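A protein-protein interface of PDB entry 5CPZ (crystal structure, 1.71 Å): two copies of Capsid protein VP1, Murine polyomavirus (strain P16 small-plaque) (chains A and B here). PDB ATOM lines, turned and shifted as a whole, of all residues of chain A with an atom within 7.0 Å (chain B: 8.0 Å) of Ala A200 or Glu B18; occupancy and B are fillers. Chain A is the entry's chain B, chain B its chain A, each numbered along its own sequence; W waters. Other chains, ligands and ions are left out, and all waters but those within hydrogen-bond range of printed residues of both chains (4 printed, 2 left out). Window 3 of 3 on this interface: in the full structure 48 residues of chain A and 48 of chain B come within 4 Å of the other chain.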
ATOM      1  N   ASP A 141      12.005   5.933 -34.258  1.00  0.00           N
ATOM      2  CA  ASP A 141      11.642   6.603 -33.007  1.00  0.00           C
ATOM      3  C   ASP A 141      12.506   6.082 -31.862  1.00  0.00           C
ATOM      4  O   ASP A 141      12.649   4.866 -31.683  1.00  0.00           O
ATOM      5  CB  ASP A 141      10.159   6.402 -32.686  1.00  0.00           C
ATOM      6  CG  ASP A 141       9.251   7.088 -33.687  1.00  0.00           C
ATOM      7  OD1 ASP A 141       9.423   8.307 -33.918  1.00  0.00           O
ATOM      8  OD2 ASP A 141       8.362   6.404 -34.239  1.00  0.00           O
ATOM      9  N   GLN A 143      13.811   6.137 -27.712  1.00  0.00           N
ATOM     10  CA  GLN A 143      13.523   6.356 -26.302  1.00  0.00           C
ATOM     11  C   GLN A 143      14.857   6.395 -25.561  1.00  0.00           C
ATOM     12  O   GLN A 143      15.677   5.478 -25.704  1.00  0.00           O
ATOM     13  CB  GLN A 143      12.639   5.221 -25.766  1.00  0.00           C
ATOM     14  CG  GLN A 143      12.507   5.165 -24.243  1.00  0.00           C
ATOM     15  CD  GLN A 143      11.736   6.348 -23.674  1.00  0.00           C
ATOM     16  OE1 GLN A 143      10.586   6.590 -24.040  1.00  0.00           O
ATOM     17  NE2 GLN A 143      12.365   7.086 -22.768  1.00  0.00           N
ATOM     18  N   LYS A 181      12.487  11.478 -25.435  1.00  0.00           N
ATOM     19  CA  LYS A 181      12.326  10.858 -26.747  1.00  0.00           C
ATOM     20  C   LYS A 181      12.978  11.696 -27.836  1.00  0.00           C
ATOM     21  O   LYS A 181      13.114  12.915 -27.701  1.00  0.00           O
ATOM     22  CB  LYS A 181      10.840  10.642 -27.063  1.00  0.00           C
ATOM     23  CG  LYS A 181      10.171   9.600 -26.182  1.00  0.00           C
ATOM     24  CD  LYS A 181       8.732   9.340 -26.589  1.00  0.00           C
ATOM     25  CE  LYS A 181       8.117   8.291 -25.675  1.00  0.00           C
ATOM     26  NZ  LYS A 181       7.009   7.574 -26.361  1.00  0.00           N
ATOM     27  N   PRO A 197      15.379   1.837 -29.517  1.00  0.00           N
ATOM     28  CA  PRO A 197      14.143   1.875 -30.293  1.00  0.00           C
ATOM     29  C   PRO A 197      12.950   2.033 -29.351  1.00  0.00           C
ATOM     30  O   PRO A 197      12.883   1.354 -28.322  1.00  0.00           O
ATOM     31  CB  PRO A 197      14.124   0.509 -30.991  1.00  0.00           C
ATOM     32  CG  PRO A 197      15.561   0.104 -31.061  1.00  0.00           C
ATOM     33  CD  PRO A 197      16.166   0.617 -29.787  1.00  0.00           C
ATOM     34  N   ASP A 198      12.043   2.945 -29.685  1.00  0.00           N
ATOM     35  CA  ASP A 198      10.878   3.232 -28.846  1.00  0.00           C
ATOM     36  C   ASP A 198       9.724   2.281 -29.192  1.00  0.00           C
ATOM     37  O   ASP A 198       9.129   2.403 -30.262  1.00  0.00           O
ATOM     38  CB  ASP A 198      10.453   4.698 -29.034  1.00  0.00           C
ATOM     39  CG  ASP A 198       9.306   5.106 -28.121  1.00  0.00           C
ATOM     40  OD1 ASP A 198       8.799   4.260 -27.356  1.00  0.00           O
ATOM     41  OD2 ASP A 198       8.902   6.284 -28.177  1.00  0.00           O
ATOM     42  N   PRO A 199       9.399   1.328 -28.289  1.00  0.00           N
ATOM     43  CA  PRO A 199       8.329   0.380 -28.610  1.00  0.00           C
ATOM     44  C   PRO A 199       6.925   0.989 -28.570  1.00  0.00           C
ATOM     45  O   PRO A 199       5.983   0.379 -29.078  1.00  0.00           O
ATOM     46  CB  PRO A 199       8.471  -0.690 -27.519  1.00  0.00           C
ATOM     47  CG  PRO A 199       9.050   0.045 -26.367  1.00  0.00           C
ATOM     48  CD  PRO A 199      10.003   1.044 -26.973  1.00  0.00           C
ATOM     49  N   ALA A 200       6.792   2.174 -27.976  1.00  0.00           N
ATOM     50  CA  ALA A 200       5.504   2.862 -27.897  1.00  0.00           C
ATOM     51  C   ALA A 200       5.182   3.630 -29.181  1.00  0.00           C
ATOM     52  O   ALA A 200       4.072   4.129 -29.344  1.00  0.00           O
ATOM     53  CB  ALA A 200       5.463   3.796 -26.694  1.00  0.00           C
ATOM     54  N   LYS A 201       6.156   3.742 -30.079  1.00  0.00           N
ATOM     55  CA  LYS A 201       5.915   4.369 -31.377  1.00  0.00           C
ATOM     56  C   LYS A 201       6.355   3.400 -32.469  1.00  0.00           C
ATOM     57  O   LYS A 201       6.023   2.216 -32.394  1.00  0.00           O
ATOM     58  CB  LYS A 201       6.601   5.740 -31.465  1.00  0.00           C
ATOM     59  CG  LYS A 201       6.082   6.736 -30.429  1.00  0.00           C
ATOM     60  CD  LYS A 201       6.758   8.094 -30.521  1.00  0.00           C
ATOM     61  CE  LYS A 201       6.245   8.895 -31.710  1.00  0.00           C
ATOM     62  NZ  LYS A 201       6.792  10.281 -31.706  1.00  0.00           N
ATOM     63  N   ASN A 202       7.074   3.883 -33.481  1.00  0.00           N
ATOM     64  CA  ASN A 202       7.575   3.013 -34.556  1.00  0.00           C
ATOM     65  C   ASN A 202       6.507   2.141 -35.228  1.00  0.00           C
ATOM     66  O   ASN A 202       6.755   0.984 -35.562  1.00  0.00           O
ATOM     67  CB  ASN A 202       8.750   2.157 -34.052  1.00  0.00           C
ATOM     68  CG  ASN A 202      10.025   2.964 -33.912  1.00  0.00           C
ATOM     69  OD1 ASN A 202      10.444   3.626 -34.853  1.00  0.00           O
ATOM     70  ND2 ASN A 202      10.643   2.915 -32.741  1.00  0.00           N
ATOM     71  N   GLU A 203       5.324   2.714 -35.439  1.00  0.00           N
ATOM     72  CA  GLU A 203       4.241   2.000 -36.114  1.00  0.00           C
ATOM     73  C   GLU A 203       4.576   1.737 -37.582  1.00  0.00           C
ATOM     74  O   GLU A 203       4.041   0.811 -38.193  1.00  0.00           O
ATOM     75  CB  GLU A 203       2.922   2.775 -36.003  1.00  0.00           C
ATOM     76  CG  GLU A 203       2.339   2.834 -34.592  1.00  0.00           C
ATOM     77  CD  GLU A 203       1.905   1.474 -34.048  1.00  0.00           C
ATOM     78  OE1 GLU A 203       1.789   1.345 -32.812  1.00  0.00           O
ATOM     79  OE2 GLU A 203       1.675   0.532 -34.842  1.00  0.00           O
ATOM     80  N   TYR A 207      11.983  -2.982 -36.341  1.00  0.00           N
ATOM     81  CA  TYR A 207      13.345  -3.083 -35.808  1.00  0.00           C
ATOM     82  C   TYR A 207      13.589  -4.428 -35.120  1.00  0.00           C
ATOM     83  O   TYR A 207      12.659  -5.064 -34.632  1.00  0.00           O
ATOM     84  CB  TYR A 207      13.686  -1.903 -34.882  1.00  0.00           C
ATOM     85  CG  TYR A 207      12.837  -1.806 -33.632  1.00  0.00           C
ATOM     86  CD1 TYR A 207      13.134  -2.566 -32.495  1.00  0.00           C
ATOM     87  CD2 TYR A 207      11.751  -0.938 -33.580  1.00  0.00           C
ATOM     88  CE1 TYR A 207      12.354  -2.477 -31.350  1.00  0.00           C
ATOM     89  CE2 TYR A 207      10.977  -0.832 -32.440  1.00  0.00           C
ATOM     90  CZ  TYR A 207      11.275  -1.605 -31.335  1.00  0.00           C
ATOM     91  OH  TYR A 207      10.496  -1.481 -30.221  1.00  0.00           O
ATOM     92  N   THR B  15     -10.153  -3.359 -28.545  1.00  0.00           N
ATOM     93  CA  THR B  15      -9.359  -2.239 -28.057  1.00  0.00           C
ATOM     94  C   THR B  15      -7.894  -2.658 -27.905  1.00  0.00           C
ATOM     95  O   THR B  15      -7.587  -3.848 -27.798  1.00  0.00           O
ATOM     96  CB  THR B  15      -9.941  -1.652 -26.743  1.00  0.00           C
ATOM     97  OG1 THR B  15      -9.412  -0.340 -26.520  1.00  0.00           O
ATOM     98  CG2 THR B  15      -9.653  -2.551 -25.529  1.00  0.00           C
ATOM     99  N   GLU B  16      -6.996  -1.678 -27.934  1.00  0.00           N
ATOM    100  CA  GLU B  16      -5.585  -1.918 -27.656  1.00  0.00           C
ATOM    101  C   GLU B  16      -5.168  -0.989 -26.543  1.00  0.00           C
ATOM    102  O   GLU B  16      -5.494   0.201 -26.570  1.00  0.00           O
ATOM    103  CB  GLU B  16      -4.722  -1.656 -28.888  1.00  0.00           C
ATOM    104  CG  GLU B  16      -4.791  -2.738 -29.951  1.00  0.00           C
ATOM    105  CD  GLU B  16      -3.816  -2.511 -31.095  1.00  0.00           C
ATOM    106  OE1 GLU B  16      -2.780  -1.836 -30.896  1.00  0.00           O
ATOM    107  OE2 GLU B  16      -4.087  -3.019 -32.204  1.00  0.00           O
ATOM    108  N   ILE B  17      -4.467  -1.527 -25.552  1.00  0.00           N
ATOM    109  CA  ILE B  17      -3.915  -0.673 -24.511  1.00  0.00           C
ATOM    110  C   ILE B  17      -2.423  -0.902 -24.341  1.00  0.00           C
ATOM    111  O   ILE B  17      -1.919  -2.009 -24.554  1.00  0.00           O
ATOM    112  CB  ILE B  17      -4.672  -0.770 -23.165  1.00  0.00           C
ATOM    113  CG1 ILE B  17      -4.665  -2.191 -22.617  1.00  0.00           C
ATOM    114  CG2 ILE B  17      -6.101  -0.253 -23.308  1.00  0.00           C
ATOM    115  CD1 ILE B  17      -5.223  -2.274 -21.217  1.00  0.00           C
ATOM    116  N   GLU B  18      -1.727   0.170 -23.988  1.00  0.00           N
ATOM    117  CA  GLU B  18      -0.290   0.086 -23.794  1.00  0.00           C
ATOM    118  C   GLU B  18       0.132   0.636 -22.448  1.00  0.00           C
ATOM    119  O   GLU B  18      -0.531   1.506 -21.867  1.00  0.00           O
ATOM    120  CB  GLU B  18       0.476   0.760 -24.942  1.00  0.00           C
ATOM    121  CG  GLU B  18       0.243   2.254 -25.078  1.00  0.00           C
ATOM    122  CD  GLU B  18       1.275   2.934 -25.958  1.00  0.00           C
ATOM    123  OE1 GLU B  18       1.604   4.103 -25.666  1.00  0.00           O
ATOM    124  OE2 GLU B  18       1.761   2.308 -26.927  1.00  0.00           O
ATOM    125  N   ALA B  19       1.239   0.102 -21.943  1.00  0.00           N
ATOM    126  CA  ALA B  19       1.771   0.527 -20.673  1.00  0.00           C
ATOM    127  C   ALA B  19       3.234   0.145 -20.567  1.00  0.00           C
ATOM    128  O   ALA B  19       3.684  -0.802 -21.219  1.00  0.00           O
ATOM    129  CB  ALA B  19       0.981  -0.098 -19.528  1.00  0.00           C
ATOM    130  N   PHE B  20       3.963   0.925 -19.781  1.00  0.00           N
ATOM    131  CA  PHE B  20       5.300   0.530 -19.372  1.00  0.00           C
ATOM    132  C   PHE B  20       5.340   0.359 -17.865  1.00  0.00           C
ATOM    133  O   PHE B  20       4.715   1.112 -17.113  1.00  0.00           O
ATOM    134  CB  PHE B  20       6.379   1.504 -19.866  1.00  0.00           C
ATOM    135  CG  PHE B  20       6.250   2.900 -19.323  1.00  0.00           C
ATOM    136  CD1 PHE B  20       5.433   3.835 -19.954  1.00  0.00           C
ATOM    137  CD2 PHE B  20       6.965   3.293 -18.193  1.00  0.00           C
ATOM    138  CE1 PHE B  20       5.316   5.126 -19.455  1.00  0.00           C
ATOM    139  CE2 PHE B  20       6.855   4.586 -17.692  1.00  0.00           C
ATOM    140  CZ  PHE B  20       6.026   5.497 -18.325  1.00  0.00           C
ATOM    141  N   LEU B  21       6.058  -0.670 -17.434  1.00  0.00           N
ATOM    142  CA  LEU B  21       6.269  -0.898 -16.017  1.00  0.00           C
ATOM    143  C   LEU B  21       7.744  -0.702 -15.721  1.00  0.00           C
ATOM    144  O   LEU B  21       8.597  -1.409 -16.264  1.00  0.00           O
ATOM    145  CB  LEU B  21       5.810  -2.304 -15.607  1.00  0.00           C
ATOM    146  CG  LEU B  21       4.322  -2.489 -15.288  1.00  0.00           C
ATOM    147  CD1 LEU B  21       3.430  -2.258 -16.503  1.00  0.00           C
ATOM    148  CD2 LEU B  21       4.086  -3.875 -14.708  1.00  0.00           C
ATOM    149  N   LEU B  71      -4.789  -2.040 -14.999  1.00  0.00           N
ATOM    150  CA  LEU B  71      -5.299  -1.052 -15.940  1.00  0.00           C
ATOM    151  C   LEU B  71      -6.805  -1.182 -16.071  1.00  0.00           C
ATOM    152  O   LEU B  71      -7.332  -2.291 -16.176  1.00  0.00           O
ATOM    153  CB  LEU B  71      -4.637  -1.206 -17.314  1.00  0.00           C
ATOM    154  CG  LEU B  71      -3.105  -1.196 -17.393  1.00  0.00           C
ATOM    155  CD1 LEU B  71      -2.674  -1.384 -18.838  1.00  0.00           C
ATOM    156  CD2 LEU B  71      -2.513   0.087 -16.821  1.00  0.00           C
ATOM    157  N   LYS B  94       2.177  -7.652 -27.244  1.00  0.00           N
ATOM    158  CA  LYS B  94       3.532  -7.392 -27.690  1.00  0.00           C
ATOM    159  C   LYS B  94       4.260  -6.794 -26.506  1.00  0.00           C
ATOM    160  O   LYS B  94       3.838  -5.773 -25.953  1.00  0.00           O
ATOM    161  CB  LYS B  94       3.535  -6.450 -28.894  1.00  0.00           C
ATOM    162  CG  LYS B  94       2.842  -7.063 -30.099  1.00  0.00           C
ATOM    163  CD  LYS B  94       2.725  -6.085 -31.251  1.00  0.00           C
ATOM    164  CE  LYS B  94       3.942  -6.161 -32.151  1.00  0.00           C
ATOM    165  NZ  LYS B  94       3.717  -5.411 -33.418  1.00  0.00           N
ATOM    166  N   GLU B  96       8.209  -5.939 -24.643  1.00  0.00           N
ATOM    167  CA  GLU B  96       9.614  -5.667 -24.924  1.00  0.00           C
ATOM    168  C   GLU B  96      10.304  -5.117 -23.682  1.00  0.00           C
ATOM    169  O   GLU B  96       9.734  -4.300 -22.962  1.00  0.00           O
ATOM    170  CB  GLU B  96       9.708  -4.660 -26.076  1.00  0.00           C
ATOM    171  CG  GLU B  96      11.115  -4.353 -26.562  1.00  0.00           C
ATOM    172  CD  GLU B  96      11.110  -3.643 -27.903  1.00  0.00           C
ATOM    173  OE1 GLU B  96      10.284  -3.993 -28.769  1.00  0.00           O
ATOM    174  OE2 GLU B  96      11.930  -2.737 -28.093  1.00  0.00           O
ATOM    175  N   VAL B  98      13.187  -2.727 -22.527  1.00  0.00           N
ATOM    176  CA  VAL B  98      13.821  -1.578 -23.184  1.00  0.00           C
ATOM    177  C   VAL B  98      15.077  -1.145 -22.439  1.00  0.00           C
ATOM    178  O   VAL B  98      15.098  -1.124 -21.205  1.00  0.00           O
ATOM    179  CB  VAL B  98      12.847  -0.377 -23.271  1.00  0.00           C
ATOM    180  CG1 VAL B  98      13.487   0.820 -23.982  1.00  0.00           C
ATOM    181  CG2 VAL B  98      11.577  -0.788 -23.995  1.00  0.00           C
ATOM    182  N   ASN B 225       9.941  -5.087 -32.336  1.00  0.00           N
ATOM    183  CA  ASN B 225       8.527  -4.713 -32.337  1.00  0.00           C
ATOM    184  C   ASN B 225       7.675  -5.606 -33.241  1.00  0.00           C
ATOM    185  O   ASN B 225       6.534  -5.263 -33.573  1.00  0.00           O
ATOM    186  CB  ASN B 225       8.349  -3.216 -32.679  1.00  0.00           C
ATOM    187  CG  ASN B 225       8.773  -2.865 -34.098  1.00  0.00           C
ATOM    188  OD1 ASN B 225       9.527  -3.599 -34.750  1.00  0.00           O
ATOM    189  ND2 ASN B 225       8.282  -1.726 -34.590  1.00  0.00           N
ATOM    190  N   LEU B 246      -7.405  -5.178 -16.026  1.00  0.00           N
ATOM    191  CA  LEU B 246      -6.339  -5.944 -16.679  1.00  0.00           C
ATOM    192  C   LEU B 246      -5.071  -5.858 -15.842  1.00  0.00           C
ATOM    193  O   LEU B 246      -4.621  -4.760 -15.501  1.00  0.00           O
ATOM    194  CB  LEU B 246      -6.062  -5.411 -18.089  1.00  0.00           C
ATOM    195  CG  LEU B 246      -4.936  -6.100 -18.877  1.00  0.00           C
ATOM    196  CD1 LEU B 246      -5.300  -7.535 -19.226  1.00  0.00           C
ATOM    197  CD2 LEU B 246      -4.634  -5.320 -20.146  1.00  0.00           C
ATOM    198  N   LEU B 248      -1.053  -6.508 -15.316  1.00  0.00           N
ATOM    199  CA  LEU B 248       0.265  -6.700 -15.918  1.00  0.00           C
ATOM    200  C   LEU B 248       1.282  -6.874 -14.801  1.00  0.00           C
ATOM    201  O   LEU B 248       1.291  -6.110 -13.841  1.00  0.00           O
ATOM    202  CB  LEU B 248       0.654  -5.482 -16.765  1.00  0.00           C
ATOM    203  CG  LEU B 248      -0.372  -5.011 -17.802  1.00  0.00           C
ATOM    204  CD1 LEU B 248       0.176  -3.796 -18.538  1.00  0.00           C
ATOM    205  CD2 LEU B 248      -0.715  -6.138 -18.773  1.00  0.00           C
ATOM    206  N   TYR B 273       7.782  -2.839 -21.689  1.00  0.00           N
ATOM    207  CA  TYR B 273       6.640  -2.307 -22.426  1.00  0.00           C
ATOM    208  C   TYR B 273       5.632  -3.424 -22.693  1.00  0.00           C
ATOM    209  O   TYR B 273       6.022  -4.566 -22.946  1.00  0.00           O
ATOM    210  CB  TYR B 273       7.132  -1.731 -23.751  1.00  0.00           C
ATOM    211  CG  TYR B 273       6.049  -1.319 -24.728  1.00  0.00           C
ATOM    212  CD1 TYR B 273       5.426  -0.083 -24.619  1.00  0.00           C
ATOM    213  CD2 TYR B 273       5.666  -2.166 -25.771  1.00  0.00           C
ATOM    214  CE1 TYR B 273       4.444   0.308 -25.518  1.00  0.00           C
ATOM    215  CE2 TYR B 273       4.685  -1.790 -26.676  1.00  0.00           C
ATOM    216  CZ  TYR B 273       4.081  -0.550 -26.545  1.00  0.00           C
ATOM    217  OH  TYR B 273       3.113  -0.170 -27.443  1.00  0.00           O
ATOM    218  N   PHE B 274       4.344  -3.087 -22.634  1.00  0.00           N
ATOM    219  CA  PHE B 274       3.266  -4.018 -22.985  1.00  0.00           C
ATOM    220  C   PHE B 274       2.304  -3.320 -23.937  1.00  0.00           C
ATOM    221  O   PHE B 274       1.910  -2.171 -23.688  1.00  0.00           O
ATOM    222  CB  PHE B 274       2.418  -4.393 -21.760  1.00  0.00           C
ATOM    223  CG  PHE B 274       3.124  -5.186 -20.689  1.00  0.00           C
ATOM    224  CD1 PHE B 274       3.992  -4.567 -19.790  1.00  0.00           C
ATOM    225  CD2 PHE B 274       2.837  -6.540 -20.513  1.00  0.00           C
ATOM    226  CE1 PHE B 274       4.592  -5.294 -18.770  1.00  0.00           C
ATOM    227  CE2 PHE B 274       3.440  -7.270 -19.493  1.00  0.00           C
ATOM    228  CZ  PHE B 274       4.317  -6.643 -18.622  1.00  0.00           C
ATOM    229  N   LYS B 275       1.933  -3.993 -25.030  1.00  0.00           N
ATOM    230  CA  LYS B 275       0.812  -3.550 -25.862  1.00  0.00           C
ATOM    231  C   LYS B 275      -0.163  -4.718 -25.976  1.00  0.00           C
ATOM    232  O   LYS B 275       0.130  -5.723 -26.627  1.00  0.00           O
ATOM    233  CB  LYS B 275       1.282  -3.063 -27.242  1.00  0.00           C
ATOM    234  CG  LYS B 275       0.161  -2.543 -28.143  1.00  0.00           C
ATOM    235  CD  LYS B 275       0.676  -1.599 -29.223  1.00  0.00           C
ATOM    236  CE  LYS B 275       1.505  -2.315 -30.281  1.00  0.00           C
ATOM    237  NZ  LYS B 275       1.982  -1.385 -31.344  1.00  0.00           N
ATOM    238  N   ILE B 276      -1.314  -4.584 -25.318  1.00  0.00           N
ATOM    239  CA  ILE B 276      -2.280  -5.676 -25.209  1.00  0.00           C
ATOM    240  C   ILE B 276      -3.468  -5.431 -26.136  1.00  0.00           C
ATOM    241  O   ILE B 276      -4.051  -4.341 -26.142  1.00  0.00           O
ATOM    242  CB  ILE B 276      -2.789  -5.864 -23.753  1.00  0.00           C
ATOM    243  CG1 ILE B 276      -1.626  -5.945 -22.751  1.00  0.00           C
ATOM    244  CG2 ILE B 276      -3.658  -7.115 -23.633  1.00  0.00           C
ATOM    245  CD1 ILE B 276      -1.233  -4.613 -22.142  1.00  0.00           C
ATOM    246  N   THR B 277      -3.809  -6.444 -26.927  1.00  0.00           N
ATOM    247  CA  THR B 277      -5.006  -6.400 -27.765  1.00  0.00           C
ATOM    248  C   THR B 277      -6.114  -7.166 -27.050  1.00  0.00           C
ATOM    249  O   THR B 277      -5.918  -8.318 -26.642  1.00  0.00           O
ATOM    250  CB  THR B 277      -4.740  -7.011 -29.157  1.00  0.00           C
ATOM    251  OG1 THR B 277      -3.736  -6.238 -29.831  1.00  0.00           O
ATOM    252  CG2 THR B 277      -6.018  -7.043 -30.015  1.00  0.00           C
ATOM    253  N   LEU B 278      -7.270  -6.519 -26.894  1.00  0.00           N
ATOM    254  CA  LEU B 278      -8.422  -7.136 -26.236  1.00  0.00           C
ATOM    255  C   LEU B 278      -9.660  -7.054 -27.112  1.00  0.00           C
ATOM    256  O   LEU B 278      -9.799  -6.143 -27.929  1.00  0.00           O
ATOM    257  CB  LEU B 278      -8.707  -6.493 -24.871  1.00  0.00           C
ATOM    258  CG  LEU B 278      -7.549  -6.457 -23.863  1.00  0.00           C
ATOM    259  CD1 LEU B 278      -6.901  -5.080 -23.871  1.00  0.00           C
ATOM    260  CD2 LEU B 278      -8.032  -6.804 -22.465  1.00  0.00           C
HETATM  261  O   HOH W   1       6.507  -0.476 -32.615  1.00  0.00           O
HETATM  262  O   HOH W   2      13.988  -1.084 -27.666  1.00  0.00           O
HETATM  263  O   HOH W   3       5.665  -1.449 -36.664  1.00  0.00           O
HETATM  264  O   HOH W   4       2.265   5.418 -27.907  1.00  0.00           O
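The side-chain carboxylate (OE2) of Glu B96 sits at hydrogen-bond distance from the side-chain hydroxyl (OH) of Tyr A207.
The side-chain amide nitrogen (ND2) of Asn B225 is in hydrogen-bond range of the backbone carbonyl oxygen (O) of Asn A202, 3.3 Å away.
The backbone NH of Tyr A207 is in hydrogen-bond range of the side-chain amide oxygen of Asn B225, 3.0 Å away.
The side-chain hydroxyl of Tyr B273 lies close to the backbone carbonyl oxygen of Pro A199.
The side-chain amino group (NZ) of Lys B275 is in salt-bridge range of the side-chain carboxylate (OE1) of Glu A203, at 3.1 Å.
OE2 of Glu B18 sits at hydrogen-bond distance from OH of Tyr B273 (2.9 Å).
The side-chain amino group (NZ) of Lys B94 is in hydrogen-bond range of the backbone carbonyl oxygen (O) of Asn B225, 2.8 Å away.
The backbone NH (N) of Tyr B273 is in hydrogen-bond range of the backbone carbonyl oxygen (O) of Glu B96, 2.8 Å away.
The backbone NH (N) of Asp A141 is in hydrogen-bond range of the side-chain amide oxygen (OD1) of Asn A202, 2.8 Å away.
OD1 of Asp A198 lies within hydrogen-bond range of N of Ala A200, 3.0 Å away.
O of Asp A198 sits at hydrogen-bond distance from ND2 of Asn A202 (2.9 Å).
Water W4 bridges O of Ala A200 and OE1 of Glu B18.
Water W2 lies within hydrogen-bond range of OE2 of Glu B96 (2.7 Å) and O of Pro A197 (2.8 Å).
Water W1 lies within hydrogen-bond range of O of Lys A201, ND2 of Asn B225 and O of Asn A202.
Water W3 lies within hydrogen-bond range of the backbone carbonyl oxygen of Asn A202 (2.9 Å), the backbone carbonyl oxygen of Glu A203 (3.2 Å) and the side-chain amide nitrogen of Asn B225 (3.4 Å).
Among the printed residues, merely in contact across the chains: Pro A199 with Glu B96 (3.97 Å), Pro A199 with Val B98 (3.6 Å), Ala A200 with Glu B18 (3.8 Å) and Ala A200 with Tyr B273 (3.6 Å).
No position is printed for both chains.
Of the 9 pairs that touch across the chains among the printed residues, none has its exchanged pair printed and touching as well.
Of the 11 printed residues of chain A, 5 touch a printed residue of chain B.
Hydrophobic or aromatic side chains of chain A within 4 Å of the printed part of chain B: Pro A199, Ala A200 and Tyr A207.
Along chain A the printed residues that touch a printed residue of chain B span positions 199 to 207.
Of the 20 printed residues of chain B, 6 touch a printed residue of chain A.
Among the printed residues, Asp or Glu carboxylates within 4 Å of a Lys or Arg side-chain nitrogen of the other chain: Glu A203 with Lys B275 (3.1 Å).
Printed residues of chain B within 4 Å of Pro A199: Glu B96 (3.97 Å), Val B98 (3.6 Å) and Tyr B273 (3.3 Å).
Of the printed residues of chain B, Glu A203 touches Lys B275 (3.1 Å).
Glu B16 touches none of the printed residues of chain A.
Printed residues of chain A within 4 Å of Glu B18: Ala A200 (3.8 Å).
Of the printed residues of chain A, Glu B96 touches Pro A199 (3.97 Å) and Tyr A207 (2.9 Å).
Of the printed residues of chain A, Asn B225 touches Asn A202 (3.3 Å) and Tyr A207 (3.0 Å).
Printed residues of chain A within 4 Å of Tyr B273: Pro A199 (3.3 Å) and Ala A200 (3.6 Å).
The nearest printed residue of chain B that does not touch Ala A200 is Lys B275 (6.2 Å).
The nearest printed residue of chain A that does not touch Glu B18 is Pro A199 (5.1 Å).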
